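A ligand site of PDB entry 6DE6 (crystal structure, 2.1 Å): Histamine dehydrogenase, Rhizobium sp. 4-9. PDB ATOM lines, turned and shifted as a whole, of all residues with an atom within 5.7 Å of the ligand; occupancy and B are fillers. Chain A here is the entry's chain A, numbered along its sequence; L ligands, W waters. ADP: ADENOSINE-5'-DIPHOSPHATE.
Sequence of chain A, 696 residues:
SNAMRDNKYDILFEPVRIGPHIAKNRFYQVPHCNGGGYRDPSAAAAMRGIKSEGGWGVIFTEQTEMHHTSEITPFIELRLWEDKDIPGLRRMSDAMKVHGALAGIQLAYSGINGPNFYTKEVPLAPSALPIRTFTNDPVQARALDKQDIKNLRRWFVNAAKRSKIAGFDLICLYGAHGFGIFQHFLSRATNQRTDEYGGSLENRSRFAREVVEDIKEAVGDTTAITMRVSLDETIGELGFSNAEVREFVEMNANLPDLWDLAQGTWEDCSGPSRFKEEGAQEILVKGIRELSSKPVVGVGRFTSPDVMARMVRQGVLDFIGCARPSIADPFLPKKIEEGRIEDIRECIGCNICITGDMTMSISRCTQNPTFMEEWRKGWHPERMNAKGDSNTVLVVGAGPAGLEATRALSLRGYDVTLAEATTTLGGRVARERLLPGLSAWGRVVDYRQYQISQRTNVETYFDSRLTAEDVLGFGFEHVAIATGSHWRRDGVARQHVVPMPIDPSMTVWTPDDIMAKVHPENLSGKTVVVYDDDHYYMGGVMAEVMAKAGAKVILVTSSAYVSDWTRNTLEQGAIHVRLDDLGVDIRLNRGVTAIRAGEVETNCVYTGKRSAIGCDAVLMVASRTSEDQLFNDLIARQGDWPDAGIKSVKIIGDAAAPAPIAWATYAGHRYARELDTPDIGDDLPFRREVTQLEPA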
ATOM      1  N   VAL A 396     -17.860 -23.628  14.740  1.00  0.00           N
ATOM      2  CA  VAL A 396     -19.268 -23.358  14.479  1.00  0.00           C
ATOM      3  C   VAL A 396     -20.108 -24.398  15.208  1.00  0.00           C
ATOM      4  O   VAL A 396     -20.137 -25.573  14.829  1.00  0.00           O
ATOM      5  CB  VAL A 396     -19.589 -23.344  12.976  1.00  0.00           C
ATOM      6  CG1 VAL A 396     -21.010 -22.805  12.770  1.00  0.00           C
ATOM      7  CG2 VAL A 396     -18.563 -22.526  12.233  1.00  0.00           C
ATOM      8  N   GLY A 397     -20.821 -23.929  16.236  1.00  0.00           N
ATOM      9  CA  GLY A 397     -21.676 -24.753  17.063  1.00  0.00           C
ATOM     10  C   GLY A 397     -21.068 -24.942  18.426  1.00  0.00           C
ATOM     11  O   GLY A 397     -19.905 -25.326  18.545  1.00  0.00           O
ATOM     12  N   ALA A 398     -21.845 -24.667  19.483  1.00  0.00           N
ATOM     13  CA  ALA A 398     -21.382 -24.780  20.859  1.00  0.00           C
ATOM     14  C   ALA A 398     -22.076 -25.924  21.590  1.00  0.00           C
ATOM     15  O   ALA A 398     -22.542 -25.772  22.717  1.00  0.00           O
ATOM     16  CB  ALA A 398     -21.592 -23.467  21.606  1.00  0.00           C
ATOM     17  N   GLY A 399     -22.176 -27.082  20.930  1.00  0.00           N
ATOM     18  CA  GLY A 399     -22.509 -28.305  21.616  1.00  0.00           C
ATOM     19  C   GLY A 399     -21.277 -28.842  22.293  1.00  0.00           C
ATOM     20  O   GLY A 399     -20.208 -28.200  22.331  1.00  0.00           O
ATOM     21  N   PRO A 400     -21.392 -30.045  22.863  1.00  0.00           N
ATOM     22  CA  PRO A 400     -20.214 -30.670  23.491  1.00  0.00           C
ATOM     23  C   PRO A 400     -19.017 -30.730  22.540  1.00  0.00           C
ATOM     24  O   PRO A 400     -17.884 -30.510  22.979  1.00  0.00           O
ATOM     25  CB  PRO A 400     -20.738 -32.062  23.890  1.00  0.00           C
ATOM     26  CG  PRO A 400     -21.954 -32.276  23.057  1.00  0.00           C
ATOM     27  CD  PRO A 400     -22.561 -30.922  22.886  1.00  0.00           C
ATOM     28  N   ALA A 401     -19.243 -30.975  21.253  1.00  0.00           N
ATOM     29  CA  ALA A 401     -18.119 -31.037  20.311  1.00  0.00           C
ATOM     30  C   ALA A 401     -17.457 -29.678  20.146  1.00  0.00           C
ATOM     31  O   ALA A 401     -16.245 -29.533  20.314  1.00  0.00           O
ATOM     32  CB  ALA A 401     -18.586 -31.573  18.967  1.00  0.00           C
ATOM     33  N   GLY A 402     -18.242 -28.667  19.792  1.00  0.00           N
ATOM     34  CA  GLY A 402     -17.664 -27.340  19.590  1.00  0.00           C
ATOM     35  C   GLY A 402     -17.051 -26.763  20.846  1.00  0.00           C
ATOM     36  O   GLY A 402     -15.985 -26.138  20.800  1.00  0.00           O
ATOM     37  N   ALA A 419     -18.982 -19.545  17.333  1.00  0.00           N
ATOM     38  CA  ALA A 419     -20.247 -19.023  16.859  1.00  0.00           C
ATOM     39  C   ALA A 419     -21.351 -20.021  17.162  1.00  0.00           C
ATOM     40  O   ALA A 419     -21.232 -21.194  16.799  1.00  0.00           O
ATOM     41  CB  ALA A 419     -20.183 -18.744  15.348  1.00  0.00           C
ATOM     42  N   GLU A 420     -22.424 -19.553  17.813  1.00  0.00           N
ATOM     43  CA  GLU A 420     -23.560 -20.379  18.186  1.00  0.00           C
ATOM     44  C   GLU A 420     -24.868 -19.779  17.682  1.00  0.00           C
ATOM     45  O   GLU A 420     -25.115 -18.587  17.842  1.00  0.00           O
ATOM     46  CB  GLU A 420     -23.641 -20.530  19.714  1.00  0.00           C
ATOM     47  CG  GLU A 420     -24.997 -21.080  20.247  1.00  0.00           C
ATOM     48  CD  GLU A 420     -25.391 -22.453  19.670  1.00  0.00           C
ATOM     49  OE1 GLU A 420     -24.490 -23.248  19.302  1.00  0.00           O
ATOM     50  OE2 GLU A 420     -26.612 -22.742  19.598  1.00  0.00           O
ATOM     51  N   ALA A 421     -25.718 -20.623  17.108  1.00  0.00           N
ATOM     52  CA  ALA A 421     -26.950 -20.137  16.484  1.00  0.00           C
ATOM     53  C   ALA A 421     -27.994 -19.666  17.495  1.00  0.00           C
ATOM     54  O   ALA A 421     -28.776 -18.757  17.191  1.00  0.00           O
ATOM     55  CB  ALA A 421     -27.532 -21.236  15.584  1.00  0.00           C
ATOM     56  N   THR A 422     -28.069 -20.269  18.686  1.00  0.00           N
ATOM     57  CA  THR A 422     -29.070 -19.869  19.670  1.00  0.00           C
ATOM     58  C   THR A 422     -28.446 -18.894  20.674  1.00  0.00           C
ATOM     59  O   THR A 422     -27.360 -18.368  20.463  1.00  0.00           O
ATOM     60  CB  THR A 422     -29.652 -21.102  20.360  1.00  0.00           C
ATOM     61  OG1 THR A 422     -28.724 -21.580  21.348  1.00  0.00           O
ATOM     62  CG2 THR A 422     -29.949 -22.194  19.353  1.00  0.00           C
ATOM     63  N   THR A 424     -27.777 -19.881  23.809  1.00  0.00           N
ATOM     64  CA  THR A 424     -27.330 -20.767  24.871  1.00  0.00           C
ATOM     65  C   THR A 424     -26.145 -21.635  24.454  1.00  0.00           C
ATOM     66  O   THR A 424     -26.100 -22.143  23.334  1.00  0.00           O
ATOM     67  CB  THR A 424     -28.507 -21.683  25.287  1.00  0.00           C
ATOM     68  OG1 THR A 424     -29.625 -20.868  25.675  1.00  0.00           O
ATOM     69  CG2 THR A 424     -28.104 -22.627  26.399  1.00  0.00           C
ATOM     70  N   GLY A 426     -24.139 -25.195  24.845  1.00  0.00           N
ATOM     71  CA  GLY A 426     -24.312 -26.581  25.253  1.00  0.00           C
ATOM     72  C   GLY A 426     -25.035 -27.501  24.279  1.00  0.00           C
ATOM     73  O   GLY A 426     -24.970 -28.730  24.452  1.00  0.00           O
ATOM     74  N   GLY A 427     -25.710 -26.964  23.276  1.00  0.00           N
ATOM     75  CA  GLY A 427     -26.356 -27.784  22.264  1.00  0.00           C
ATOM     76  C   GLY A 427     -27.258 -28.832  22.888  1.00  0.00           C
ATOM     77  O   GLY A 427     -28.100 -28.544  23.739  1.00  0.00           O
ATOM     78  N   ARG A 428     -27.071 -30.096  22.458  1.00  0.00           N
ATOM     79  CA  ARG A 428     -27.924 -31.172  22.969  1.00  0.00           C
ATOM     80  C   ARG A 428     -27.827 -31.320  24.478  1.00  0.00           C
ATOM     81  O   ARG A 428     -28.795 -31.743  25.126  1.00  0.00           O
ATOM     82  CB  ARG A 428     -27.560 -32.502  22.292  1.00  0.00           C
ATOM     83  CG  ARG A 428     -26.142 -33.023  22.682  1.00  0.00           C
ATOM     84  CD  ARG A 428     -25.799 -34.226  21.871  1.00  0.00           C
ATOM     85  NE  ARG A 428     -26.502 -35.415  22.340  1.00  0.00           N
ATOM     86  CZ  ARG A 428     -26.152 -36.659  22.016  1.00  0.00           C
ATOM     87  NH1 ARG A 428     -25.124 -36.863  21.194  1.00  0.00           N
ATOM     88  NH2 ARG A 428     -26.812 -37.693  22.505  1.00  0.00           N
ATOM     89  N   VAL A 429     -26.677 -31.008  25.069  1.00  0.00           N
ATOM     90  CA  VAL A 429     -26.572 -31.213  26.509  1.00  0.00           C
ATOM     91  C   VAL A 429     -27.364 -30.152  27.255  1.00  0.00           C
ATOM     92  O   VAL A 429     -27.909 -30.435  28.329  1.00  0.00           O
ATOM     93  CB  VAL A 429     -25.111 -31.214  26.995  1.00  0.00           C
ATOM     94  CG1 VAL A 429     -25.032 -31.468  28.531  1.00  0.00           C
ATOM     95  CG2 VAL A 429     -24.350 -32.215  26.229  1.00  0.00           C
ATOM     96  N   ARG A 431     -30.160 -29.028  26.400  1.00  0.00           N
ATOM     97  CA  ARG A 431     -31.535 -29.525  26.351  1.00  0.00           C
ATOM     98  C   ARG A 431     -31.698 -30.845  27.127  1.00  0.00           C
ATOM     99  O   ARG A 431     -32.635 -30.995  27.910  1.00  0.00           O
ATOM    100  CB  ARG A 431     -31.947 -29.701  24.887  1.00  0.00           C
ATOM    101  CG  ARG A 431     -31.899 -28.387  24.094  1.00  0.00           C
ATOM    102  CD  ARG A 431     -32.260 -28.549  22.616  1.00  0.00           C
ATOM    103  NE  ARG A 431     -31.189 -29.189  21.833  1.00  0.00           N
ATOM    104  CZ  ARG A 431     -31.323 -30.312  21.127  1.00  0.00           C
ATOM    105  NH1 ARG A 431     -32.498 -30.961  21.067  1.00  0.00           N
ATOM    106  NH2 ARG A 431     -30.266 -30.782  20.461  1.00  0.00           N
ATOM    107  N   SER A 464     -26.047 -16.395  16.043  1.00  0.00           N
ATOM    108  CA  SER A 464     -25.297 -16.361  14.787  1.00  0.00           C
ATOM    109  C   SER A 464     -25.343 -17.724  14.099  1.00  0.00           C
ATOM    110  O   SER A 464     -24.371 -18.485  14.156  1.00  0.00           O
ATOM    111  CB  SER A 464     -23.861 -15.925  15.052  1.00  0.00           C
ATOM    112  OG  SER A 464     -23.797 -14.822  15.923  1.00  0.00           O
ATOM    113  N   ARG A 465     -26.451 -18.032  13.447  1.00  0.00           N
ATOM    114  CA  ARG A 465     -26.497 -19.218  12.573  1.00  0.00           C
ATOM    115  C   ARG A 465     -25.724 -18.915  11.293  1.00  0.00           C
ATOM    116  O   ARG A 465     -26.184 -18.171  10.427  1.00  0.00           O
ATOM    117  CB  ARG A 465     -27.942 -19.615  12.294  1.00  0.00           C
ATOM    118  CG  ARG A 465     -28.071 -20.919  11.563  1.00  0.00           C
ATOM    119  CD  ARG A 465     -29.509 -21.207  11.174  1.00  0.00           C
ATOM    120  NE  ARG A 465     -29.983 -20.306  10.121  1.00  0.00           N
ATOM    121  N   LEU A 466     -24.479 -19.389  11.208  1.00  0.00           N
ATOM    122  CA  LEU A 466     -23.612 -19.036  10.100  1.00  0.00           C
ATOM    123  C   LEU A 466     -24.016 -19.733   8.791  1.00  0.00           C
ATOM    124  O   LEU A 466     -24.424 -20.904   8.775  1.00  0.00           O
ATOM    125  CB  LEU A 466     -22.165 -19.376  10.434  1.00  0.00           C
ATOM    126  CG  LEU A 466     -21.638 -18.649  11.686  1.00  0.00           C
ATOM    127  CD1 LEU A 466     -20.143 -18.774  11.744  1.00  0.00           C
ATOM    128  CD2 LEU A 466     -22.063 -17.174  11.715  1.00  0.00           C
ATOM    129  N   THR A 467     -23.886 -18.994   7.685  1.00  0.00           N
ATOM    130  CA  THR A 467     -23.903 -19.573   6.350  1.00  0.00           C
ATOM    131  C   THR A 467     -22.475 -19.693   5.831  1.00  0.00           C
ATOM    132  O   THR A 467     -21.545 -19.077   6.369  1.00  0.00           O
ATOM    133  CB  THR A 467     -24.715 -18.724   5.368  1.00  0.00           C
ATOM    134  OG1 THR A 467     -24.036 -17.493   5.186  1.00  0.00           O
ATOM    135  CG2 THR A 467     -26.080 -18.467   5.880  1.00  0.00           C
ATOM    136  N   ALA A 482     -19.267 -27.922  13.888  1.00  0.00           N
ATOM    137  CA  ALA A 482     -19.756 -28.785  14.956  1.00  0.00           C
ATOM    138  C   ALA A 482     -21.232 -28.521  15.173  1.00  0.00           C
ATOM    139  O   ALA A 482     -21.658 -28.183  16.272  1.00  0.00           O
ATOM    140  CB  ALA A 482     -18.967 -28.543  16.243  1.00  0.00           C
ATOM    141  N   THR A 483     -22.028 -28.683  14.115  1.00  0.00           N
ATOM    142  CA  THR A 483     -23.384 -28.168  14.062  1.00  0.00           C
ATOM    143  C   THR A 483     -24.434 -29.182  14.455  1.00  0.00           C
ATOM    144  O   THR A 483     -25.623 -28.904  14.311  1.00  0.00           O
ATOM    145  CB  THR A 483     -23.693 -27.632  12.657  1.00  0.00           C
ATOM    146  OG1 THR A 483     -23.189 -28.549  11.663  1.00  0.00           O
ATOM    147  CG2 THR A 483     -23.032 -26.270  12.458  1.00  0.00           C
ATOM    148  N   GLY A 484     -24.039 -30.362  14.933  1.00  0.00           N
ATOM    149  CA  GLY A 484     -24.993 -31.247  15.582  1.00  0.00           C
ATOM    150  C   GLY A 484     -25.860 -32.056  14.637  1.00  0.00           C
ATOM    151  O   GLY A 484     -25.485 -32.376  13.511  1.00  0.00           O
ATOM    152  N   SER A 485     -27.083 -32.363  15.105  1.00  0.00           N
ATOM    153  CA  SER A 485     -27.984 -33.319  14.474  1.00  0.00           C
ATOM    154  C   SER A 485     -29.392 -33.097  14.999  1.00  0.00           C
ATOM    155  O   SER A 485     -29.602 -32.424  16.015  1.00  0.00           O
ATOM    156  CB  SER A 485     -27.560 -34.765  14.769  1.00  0.00           C
ATOM    157  OG  SER A 485     -27.836 -35.060  16.129  1.00  0.00           O
ATOM    158  N   GLU A 627     -26.745 -32.372  10.937  1.00  0.00           N
ATOM    159  CA  GLU A 627     -26.877 -31.021  10.397  1.00  0.00           C
ATOM    160  C   GLU A 627     -25.549 -30.714   9.721  1.00  0.00           C
ATOM    161  O   GLU A 627     -24.588 -30.313  10.373  1.00  0.00           O
ATOM    162  CB  GLU A 627     -27.219 -30.022  11.496  1.00  0.00           C
ATOM    163  CG  GLU A 627     -27.437 -28.601  11.012  1.00  0.00           C
ATOM    164  CD  GLU A 627     -28.419 -28.553   9.860  1.00  0.00           C
ATOM    165  OE1 GLU A 627     -27.997 -28.289   8.698  1.00  0.00           O
ATOM    166  OE2 GLU A 627     -29.597 -28.864  10.136  1.00  0.00           O
ATOM    167  N   LEU A 630     -24.169 -26.580   6.133  1.00  0.00           N
ATOM    168  CA  LEU A 630     -23.113 -25.573   6.100  1.00  0.00           C
ATOM    169  C   LEU A 630     -21.822 -26.172   5.592  1.00  0.00           C
ATOM    170  O   LEU A 630     -21.162 -25.612   4.706  1.00  0.00           O
ATOM    171  CB  LEU A 630     -22.908 -24.975   7.497  1.00  0.00           C
ATOM    172  CG  LEU A 630     -21.689 -24.044   7.695  1.00  0.00           C
ATOM    173  CD1 LEU A 630     -21.736 -22.874   6.715  1.00  0.00           C
ATOM    174  CD2 LEU A 630     -21.624 -23.514   9.151  1.00  0.00           C
ATOM    175  N   ILE A 652     -17.169 -32.335  12.663  1.00  0.00           N
ATOM    176  CA  ILE A 652     -16.901 -33.125  13.868  1.00  0.00           C
ATOM    177  C   ILE A 652     -18.195 -33.297  14.659  1.00  0.00           C
ATOM    178  O   ILE A 652     -19.129 -32.485  14.566  1.00  0.00           O
ATOM    179  CB  ILE A 652     -15.821 -32.491  14.791  1.00  0.00           C
ATOM    180  CG1 ILE A 652     -16.267 -31.114  15.317  1.00  0.00           C
ATOM    181  CG2 ILE A 652     -14.497 -32.388  14.077  1.00  0.00           C
ATOM    182  CD1 ILE A 652     -15.278 -30.495  16.378  1.00  0.00           C
ATOM    183  N   GLY A 653     -18.225 -34.366  15.455  1.00  0.00           N
ATOM    184  CA  GLY A 653     -19.303 -34.631  16.371  1.00  0.00           C
ATOM    185  C   GLY A 653     -20.516 -35.198  15.667  1.00  0.00           C
ATOM    186  O   GLY A 653     -20.428 -35.883  14.648  1.00  0.00           O
ATOM    187  N   ASP A 654     -21.678 -34.913  16.244  1.00  0.00           N
ATOM    188  CA  ASP A 654     -22.924 -35.416  15.684  1.00  0.00           C
ATOM    189  C   ASP A 654     -23.119 -34.940  14.232  1.00  0.00           C
ATOM    190  O   ASP A 654     -23.769 -35.632  13.439  1.00  0.00           O
ATOM    191  CB  ASP A 654     -24.088 -34.984  16.564  1.00  0.00           C
ATOM    192  CG  ASP A 654     -24.178 -35.774  17.883  1.00  0.00           C
ATOM    193  OD1 ASP A 654     -23.841 -36.984  17.908  1.00  0.00           O
ATOM    194  OD2 ASP A 654     -24.568 -35.177  18.910  1.00  0.00           O
ATOM    195  N   ALA A 655     -22.555 -33.790  13.870  1.00  0.00           N
ATOM    196  CA  ALA A 655     -22.673 -33.369  12.474  1.00  0.00           C
ATOM    197  C   ALA A 655     -21.904 -34.287  11.525  1.00  0.00           C
ATOM    198  O   ALA A 655     -22.193 -34.315  10.322  1.00  0.00           O
ATOM    199  CB  ALA A 655     -22.193 -31.919  12.333  1.00  0.00           C
ATOM    200  N   ALA A 664     -18.741 -36.866  21.025  1.00  0.00           N
ATOM    201  CA  ALA A 664     -18.658 -35.459  20.628  1.00  0.00           C
ATOM    202  C   ALA A 664     -17.519 -34.728  21.355  1.00  0.00           C
ATOM    203  O   ALA A 664     -16.762 -33.968  20.722  1.00  0.00           O
ATOM    204  CB  ALA A 664     -19.991 -34.770  20.874  1.00  0.00           C
HETATM  205  PB  ADP L   1     -22.564 -32.124  19.204  1.00  0.00           P
HETATM  206  O1B ADP L   1     -21.721 -31.116  19.916  1.00  0.00           O
HETATM  207  O2B ADP L   1     -23.178 -33.152  20.123  1.00  0.00           O
HETATM  208  O3B ADP L   1     -21.934 -32.663  17.959  1.00  0.00           O
HETATM  209  PA  ADP L   1     -25.008 -30.517  19.302  1.00  0.00           P
HETATM  210  O1A ADP L   1     -26.219 -30.830  18.495  1.00  0.00           O
HETATM  211  O2A ADP L   1     -25.023 -30.775  20.789  1.00  0.00           O
HETATM  212  O3A ADP L   1     -23.768 -31.260  18.578  1.00  0.00           O
HETATM  213  O5' ADP L   1     -24.631 -28.974  19.078  1.00  0.00           O
HETATM  214  C5' ADP L   1     -24.809 -28.348  17.810  1.00  0.00           C
HETATM  215  C4' ADP L   1     -24.858 -26.844  18.019  1.00  0.00           C
HETATM  216  O4' ADP L   1     -24.647 -26.160  16.780  1.00  0.00           O
HETATM  217  C3' ADP L   1     -26.180 -26.313  18.586  1.00  0.00           C
HETATM  218  O3' ADP L   1     -25.859 -25.522  19.725  1.00  0.00           O
HETATM  219  C2' ADP L   1     -26.811 -25.471  17.487  1.00  0.00           C
HETATM  220  O2' ADP L   1     -27.469 -24.321  17.977  1.00  0.00           O
HETATM  221  C1' ADP L   1     -25.585 -25.077  16.706  1.00  0.00           C
HETATM  222  N9  ADP L   1     -25.744 -24.806  15.265  1.00  0.00           N
HETATM  223  C8  ADP L   1     -26.347 -25.529  14.295  1.00  0.00           C
HETATM  224  N7  ADP L   1     -26.189 -24.915  13.090  1.00  0.00           N
HETATM  225  C5  ADP L   1     -25.456 -23.810  13.303  1.00  0.00           C
HETATM  226  C6  ADP L   1     -24.912 -22.699  12.507  1.00  0.00           C
HETATM  227  N6  ADP L   1     -25.126 -22.645  11.183  1.00  0.00           N
HETATM  228  N1  ADP L   1     -24.205 -21.748  13.142  1.00  0.00           N
HETATM  229  C2  ADP L   1     -23.975 -21.762  14.464  1.00  0.00           C
HETATM  230  N3  ADP L   1     -24.435 -22.747  15.257  1.00  0.00           N
HETATM  231  C4  ADP L   1     -25.170 -23.752  14.742  1.00  0.00           C
HETATM  232  O   HOH W   1     -26.659 -24.500  22.311  1.00  0.00           O
HETATM  233  O   HOH W   2     -26.760 -33.592  18.229  1.00  0.00           O
HETATM  234  O   HOH W   3     -21.595 -31.663  15.646  1.00  0.00           O
HETATM  235  O   HOH W   4     -26.612 -25.141  10.083  1.00  0.00           O
HETATM  236  O   HOH W   5     -21.015 -28.660  18.899  1.00  0.00           O
HETATM  237  O   HOH W   6     -27.950 -28.422  15.385  1.00  0.00           O
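N of Leu 466 sits at hydrogen-bond distance from N1 of the ligand (3.1 Å).
An oxygen (O2B) of the ligand sits close to the side-chain carboxylate (OD2) of Asp 654 (2.7 Å).
The backbone NH (N) of Ala 401 is in hydrogen-bond range of an oxygen (O1B) of the ligand, at 2.8 Å.
N6 of the ligand sits at hydrogen-bond distance from O of Leu 466 (3.1 Å).
The backbone NH of Ala 421 is in hydrogen-bond range of a nitrogen (N3) of the ligand (3.1 Å).
The backbone NH (N) of Asp 654 is in hydrogen-bond range of an oxygen (O3B) of the ligand (2.8 Å).
OE2 of Glu 420 is in hydrogen-bond range of O2' of the ligand, 2.4 Å away.
O2A of the ligand sits at hydrogen-bond distance from N of Arg 428, 2.7 Å away.
The side-chain carboxylate (OD2) of Asp 654 is in salt-bridge range of the guanidinium group (NH1) of Arg 428 (2.9 Å).
The backbone NH (N) of Gly 427 sits at hydrogen-bond distance from the backbone carbonyl oxygen (O) of Ala 398, at 3.4 Å.
The side-chain hydroxyl of Thr 422 lies within hydrogen-bond range of the backbone NH of Thr 424.
N of Ala 398 is in hydrogen-bond range of OE1 of Glu 420, 3.0 Å away.
N of Gly 397 sits at hydrogen-bond distance from O of Ala 419 (2.8 Å).
N of Gly 426 is in hydrogen-bond range of O of Ala 398.
OG1 of Thr 483 lies within hydrogen-bond range of O of Glu 627 (2.6 Å).
The side-chain hydroxyl (OG1) of Thr 422 lies within hydrogen-bond range of the side-chain carboxylate (OE2) of Glu 420, 3.0 Å away.
O1B of the ligand lies close to N of Pro 400.
The backbone carbonyl oxygen (O) of Ser 464 sits close to a nitrogen (N1) of the ligand (3.4 Å).
Merely in contact with the ligand: Gly 484, Gly 397, Gly 399, Val 396, Arg 465, Gly 427, Thr 483, Ala 482, Thr 422, Ala 419, Gly 653, Ala 664, Ser 485 and Ala 398.
Hydrophobic or aromatic side chains that line the ligand: Val 396, Pro 400, Ala 401, Ala 421 and Ala 664.
Within 4 Å of the ligand: Val 396, Gly 397, Ala 398, Gly 399, Pro 400, Ala 401, Ala 419, Glu 420, Ala 421, Thr 422, Gly 427, Arg 428, Ser 464, Arg 465, Leu 466, Ala 482, Thr 483, Gly 484, Ser 485, Gly 653, Asp 654 and Ala 664.
Water W5 lies within hydrogen-bond range of O of Ala 482, O1B of the ligand, N of Gly 399 and N of Gly 402.
Water W2 lies within hydrogen-bond range of the side-chain hydroxyl of Ser 485, the side-chain carboxylate of Asp 654 and an oxygen (O1A) of the ligand.
Water W1 lies within hydrogen-bond range of the backbone carbonyl oxygen (O) of Thr 424 (2.6 Å), the backbone NH (N) of Gly 427 (2.8 Å), an oxygen (O3') of the ligand (2.9 Å) and the side-chain carboxylate (OE2) of Glu 420 (3.2 Å).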
